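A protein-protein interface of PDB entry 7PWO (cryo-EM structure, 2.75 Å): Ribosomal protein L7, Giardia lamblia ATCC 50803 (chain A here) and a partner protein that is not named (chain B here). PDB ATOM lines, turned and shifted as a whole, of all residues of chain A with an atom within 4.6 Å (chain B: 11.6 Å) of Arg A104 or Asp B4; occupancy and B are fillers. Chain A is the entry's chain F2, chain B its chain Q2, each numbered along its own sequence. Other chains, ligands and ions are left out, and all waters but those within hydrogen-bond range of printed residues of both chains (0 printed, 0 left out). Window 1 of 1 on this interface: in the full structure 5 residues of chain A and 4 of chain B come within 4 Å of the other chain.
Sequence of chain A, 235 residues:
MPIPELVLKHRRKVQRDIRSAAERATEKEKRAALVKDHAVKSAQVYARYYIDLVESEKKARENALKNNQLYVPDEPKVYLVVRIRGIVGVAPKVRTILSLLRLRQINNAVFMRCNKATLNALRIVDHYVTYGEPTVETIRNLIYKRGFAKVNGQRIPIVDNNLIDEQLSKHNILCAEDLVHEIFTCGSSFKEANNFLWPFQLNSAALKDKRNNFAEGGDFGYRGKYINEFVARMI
The guanidinium group (NH1) of Arg A104 lies close to the backbone carbonyl oxygen (O) of Asp B4 (3.1 Å).
NH1 of Arg A104 sits at hydrogen-bond distance from O of Thr B7, at 3.1 Å.
The side-chain amide nitrogen (NE2) of Gln A105 is in hydrogen-bond range of the backbone carbonyl oxygen (O) of Gly B2 (3.5 Å).
OD1 of Asp B4 lies within hydrogen-bond range of N of Lys B6 (3.5 Å).
Among the printed residues, merely in contact across the chains: Ile A87 with Gly B2, Ile A87 with Ile B3, Ser A99 with Thr B7 and Arg A104 with Ile B3.
Of chain B, only Gly B2 and Ile B3 come within 4 Å of Ile A87.
Of chain B, only Thr B7 comes within 4 Å of Ser A99.
Arg A102 touches none of the printed residues of chain B.
Leu A103 touches none of the printed residues of chain B.
Of the printed residues of chain A, Gly B2 touches Ile A87 and Gln A105.
Of the printed residues of chain A, Ile B3 touches Ile A87 (3.8 Å) and Arg A104 (3.8 Å).
Asp B4 touches just one residue of chain A: Arg A104 (3.1 Å).
Lys B10 touches none of the printed residues of chain A.
The nearest residue of chain B that does not touch Arg A104 is Ile B9 (4.1 Å).
Of the 7 printed residues of chain A, 4 touch a printed residue of chain B.
Hydrophobic or aromatic side chains of chain A within 4 Å of the printed part of chain B: Ile A87.
Among the printed residues, 7 pairs touch across the chains.
Among the printed residues, no Asp or Glu carboxylate lies within 4 Å of a Lys or Arg side-chain nitrogen of the other chain.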
ATOM      1  N   ARG A  83      10.914  15.596   7.720  1.00  0.00           N
ATOM      2  CA  ARG A  83       9.932  15.913   8.759  1.00  0.00           C
ATOM      3  C   ARG A  83      10.497  15.501  10.117  1.00  0.00           C
ATOM      4  O   ARG A  83      11.238  14.524  10.207  1.00  0.00           O
ATOM      5  CB  ARG A  83       8.599  15.209   8.467  1.00  0.00           C
ATOM      6  CG  ARG A  83       7.379  15.819   9.177  1.00  0.00           C
ATOM      7  CD  ARG A  83       6.135  14.933   9.124  1.00  0.00           C
ATOM      8  NE  ARG A  83       5.141  15.349  10.120  1.00  0.00           N
ATOM      9  CZ  ARG A  83       3.893  15.738   9.872  1.00  0.00           C
ATOM     10  NH1 ARG A  83       3.107  16.090  10.875  1.00  0.00           N
ATOM     11  NH2 ARG A  83       3.417  15.766   8.643  1.00  0.00           N
ATOM     12  N   ILE A  87       2.043  13.794  14.032  1.00  0.00           N
ATOM     13  CA  ILE A  87       0.731  14.097  13.455  1.00  0.00           C
ATOM     14  C   ILE A  87      -0.340  14.529  14.456  1.00  0.00           C
ATOM     15  O   ILE A  87      -1.449  14.878  14.031  1.00  0.00           O
ATOM     16  CB  ILE A  87       0.207  12.899  12.628  1.00  0.00           C
ATOM     17  CG1 ILE A  87      -0.295  11.778  13.548  1.00  0.00           C
ATOM     18  CG2 ILE A  87       1.252  12.421  11.633  1.00  0.00           C
ATOM     19  CD1 ILE A  87      -0.788  10.572  12.835  1.00  0.00           C
ATOM     20  N   SER A  99       1.061  17.930   3.299  1.00  0.00           N
ATOM     21  CA  SER A  99       0.544  16.907   2.395  1.00  0.00           C
ATOM     22  C   SER A  99       1.010  17.145   0.968  1.00  0.00           C
ATOM     23  O   SER A  99       1.375  16.203   0.261  1.00  0.00           O
ATOM     24  CB  SER A  99      -0.978  16.864   2.451  1.00  0.00           C
ATOM     25  OG  SER A  99      -1.528  18.059   1.940  1.00  0.00           O
ATOM     26  N   ARG A 102       4.359  16.060   0.450  1.00  0.00           N
ATOM     27  CA  ARG A 102       4.450  14.597   0.512  1.00  0.00           C
ATOM     28  C   ARG A 102       5.204  14.129   1.758  1.00  0.00           C
ATOM     29  O   ARG A 102       5.958  13.162   1.714  1.00  0.00           O
ATOM     30  CB  ARG A 102       5.087  14.002  -0.748  1.00  0.00           C
ATOM     31  CG  ARG A 102       4.344  14.233  -2.059  1.00  0.00           C
ATOM     32  CD  ARG A 102       4.785  13.191  -3.083  1.00  0.00           C
ATOM     33  NE  ARG A 102       6.151  13.408  -3.538  1.00  0.00           N
ATOM     34  CZ  ARG A 102       6.908  12.479  -4.118  1.00  0.00           C
ATOM     35  NH1 ARG A 102       6.441  11.252  -4.301  1.00  0.00           N
ATOM     36  NH2 ARG A 102       8.141  12.762  -4.501  1.00  0.00           N
ATOM     37  N   LEU A 103       4.989  14.818   2.873  1.00  0.00           N
ATOM     38  CA  LEU A 103       5.641  14.534   4.147  1.00  0.00           C
ATOM     39  C   LEU A 103       4.547  14.159   5.139  1.00  0.00           C
ATOM     40  O   LEU A 103       4.012  15.012   5.847  1.00  0.00           O
ATOM     41  CB  LEU A 103       6.443  15.732   4.610  1.00  0.00           C
ATOM     42  CG  LEU A 103       7.799  15.990   3.950  1.00  0.00           C
ATOM     43  CD1 LEU A 103       8.567  17.035   4.730  1.00  0.00           C
ATOM     44  CD2 LEU A 103       8.612  14.714   3.837  1.00  0.00           C
ATOM     45  N   ARG A 104       4.215  12.875   5.188  1.00  0.00           N
ATOM     46  CA  ARG A 104       3.067  12.412   5.943  1.00  0.00           C
ATOM     47  C   ARG A 104       3.452  11.667   7.213  1.00  0.00           C
ATOM     48  O   ARG A 104       2.584  11.431   8.053  1.00  0.00           O
ATOM     49  CB  ARG A 104       2.194  11.515   5.051  1.00  0.00           C
ATOM     50  CG  ARG A 104       1.488  12.251   3.910  1.00  0.00           C
ATOM     51  CD  ARG A 104       0.392  11.421   3.237  1.00  0.00           C
ATOM     52  NE  ARG A 104      -0.091  12.035   1.999  1.00  0.00           N
ATOM     53  CZ  ARG A 104      -1.290  12.594   1.837  1.00  0.00           C
ATOM     54  NH1 ARG A 104      -2.151  12.642   2.836  1.00  0.00           N
ATOM     55  NH2 ARG A 104      -1.625  13.115   0.667  1.00  0.00           N
ATOM     56  N   GLN A 105       4.731  11.329   7.391  1.00  0.00           N
ATOM     57  CA  GLN A 105       5.207  10.546   8.523  1.00  0.00           C
ATOM     58  C   GLN A 105       6.474  11.189   9.082  1.00  0.00           C
ATOM     59  O   GLN A 105       7.187  11.895   8.374  1.00  0.00           O
ATOM     60  CB  GLN A 105       5.453   9.098   8.101  1.00  0.00           C
ATOM     61  CG  GLN A 105       5.736   8.144   9.218  1.00  0.00           C
ATOM     62  CD  GLN A 105       5.538   6.709   8.816  1.00  0.00           C
ATOM     63  OE1 GLN A 105       6.106   6.242   7.835  1.00  0.00           O
ATOM     64  NE2 GLN A 105       4.729   5.995   9.579  1.00  0.00           N
ATOM     65  N   GLY B   2       2.539   6.599  13.479  1.00  0.00           N
ATOM     66  CA  GLY B   2       1.378   7.190  12.845  1.00  0.00           C
ATOM     67  C   GLY B   2       1.640   7.826  11.494  1.00  0.00           C
ATOM     68  O   GLY B   2       2.726   8.327  11.224  1.00  0.00           O
ATOM     69  N   ILE B   3       0.621   7.808  10.644  1.00  0.00           N
ATOM     70  CA  ILE B   3       0.682   8.356   9.296  1.00  0.00           C
ATOM     71  C   ILE B   3      -0.584   9.162   9.058  1.00  0.00           C
ATOM     72  O   ILE B   3      -1.647   8.843   9.595  1.00  0.00           O
ATOM     73  CB  ILE B   3       0.850   7.235   8.241  1.00  0.00           C
ATOM     74  CG1 ILE B   3       1.162   7.816   6.866  1.00  0.00           C
ATOM     75  CG2 ILE B   3      -0.367   6.331   8.203  1.00  0.00           C
ATOM     76  CD1 ILE B   3       1.638   6.808   5.894  1.00  0.00           C
ATOM     77  N   ASP B   4      -0.472  10.229   8.276  1.00  0.00           N
ATOM     78  CA  ASP B   4      -1.630  11.074   7.970  1.00  0.00           C
ATOM     79  C   ASP B   4      -2.147  10.723   6.580  1.00  0.00           C
ATOM     80  O   ASP B   4      -1.620  11.192   5.573  1.00  0.00           O
ATOM     81  CB  ASP B   4      -1.295  12.557   8.056  1.00  0.00           C
ATOM     82  CG  ASP B   4      -2.422  13.429   7.528  1.00  0.00           C
ATOM     83  OD1 ASP B   4      -3.588  13.200   7.918  1.00  0.00           O
ATOM     84  OD2 ASP B   4      -2.152  14.340   6.725  1.00  0.00           O
ATOM     85  N   LEU B   5      -3.199   9.922   6.530  1.00  0.00           N
ATOM     86  CA  LEU B   5      -3.844   9.555   5.279  1.00  0.00           C
ATOM     87  C   LEU B   5      -5.254  10.131   5.191  1.00  0.00           C
ATOM     88  O   LEU B   5      -6.185   9.466   4.742  1.00  0.00           O
ATOM     89  CB  LEU B   5      -3.879   8.041   5.114  1.00  0.00           C
ATOM     90  CG  LEU B   5      -2.554   7.291   5.216  1.00  0.00           C
ATOM     91  CD1 LEU B   5      -2.820   5.847   5.561  1.00  0.00           C
ATOM     92  CD2 LEU B   5      -1.728   7.418   3.944  1.00  0.00           C
ATOM     93  N   LYS B   6      -5.431  11.375   5.626  1.00  0.00           N
ATOM     94  CA  LYS B   6      -6.737  12.021   5.616  1.00  0.00           C
ATOM     95  C   LYS B   6      -6.832  13.193   4.653  1.00  0.00           C
ATOM     96  O   LYS B   6      -7.772  13.253   3.862  1.00  0.00           O
ATOM     97  CB  LYS B   6      -7.105  12.475   7.029  1.00  0.00           C
ATOM     98  CG  LYS B   6      -7.604  11.332   7.879  1.00  0.00           C
ATOM     99  CD  LYS B   6      -7.146  11.411   9.318  1.00  0.00           C
ATOM    100  CE  LYS B   6      -8.215  10.883  10.239  1.00  0.00           C
ATOM    101  NZ  LYS B   6      -7.749  10.779  11.637  1.00  0.00           N
ATOM    102  N   THR B   7      -5.885  14.128   4.684  1.00  0.00           N
ATOM    103  CA  THR B   7      -6.014  15.342   3.890  1.00  0.00           C
ATOM    104  C   THR B   7      -5.619  15.083   2.441  1.00  0.00           C
ATOM    105  O   THR B   7      -4.615  14.424   2.160  1.00  0.00           O
ATOM    106  CB  THR B   7      -5.177  16.478   4.490  1.00  0.00           C
ATOM    107  OG1 THR B   7      -5.229  17.624   3.637  1.00  0.00           O
ATOM    108  CG2 THR B   7      -3.744  16.077   4.676  1.00  0.00           C
ATOM    109  N   GLY B   8      -6.433  15.593   1.521  1.00  0.00           N
ATOM    110  CA  GLY B   8      -6.234  15.363   0.110  1.00  0.00           C
ATOM    111  C   GLY B   8      -6.716  14.025  -0.402  1.00  0.00           C
ATOM    112  O   GLY B   8      -6.557  13.749  -1.593  1.00  0.00           O
ATOM    113  N   ILE B   9      -7.298  13.189   0.454  1.00  0.00           N
ATOM    114  CA  ILE B   9      -7.770  11.856   0.094  1.00  0.00           C
ATOM    115  C   ILE B   9      -9.219  11.710   0.529  1.00  0.00           C
ATOM    116  O   ILE B   9      -9.631  12.241   1.564  1.00  0.00           O
ATOM    117  CB  ILE B   9      -6.902  10.739   0.719  1.00  0.00           C
ATOM    118  CG1 ILE B   9      -5.413  11.032   0.529  1.00  0.00           C
ATOM    119  CG2 ILE B   9      -7.285   9.380   0.169  1.00  0.00           C
ATOM    120  CD1 ILE B   9      -4.514   9.901   0.957  1.00  0.00           C
ATOM    121  N   LYS B  10      -9.994  10.976  -0.263  1.00  0.00           N
ATOM    122  CA  LYS B  10     -11.433  10.862  -0.079  1.00  0.00           C
ATOM    123  C   LYS B  10     -11.841   9.443   0.292  1.00  0.00           C
ATOM    124  O   LYS B  10     -11.055   8.499   0.227  1.00  0.00           O
ATOM    125  CB  LYS B  10     -12.178  11.311  -1.339  1.00  0.00           C
ATOM    126  CG  LYS B  10     -12.027  12.782  -1.652  1.00  0.00           C
ATOM    127  CD  LYS B  10     -12.808  13.145  -2.902  1.00  0.00           C
ATOM    128  CE  LYS B  10     -12.766  14.637  -3.201  1.00  0.00           C
ATOM    129  NZ  LYS B  10     -11.437  15.143  -3.571  1.00  0.00           N
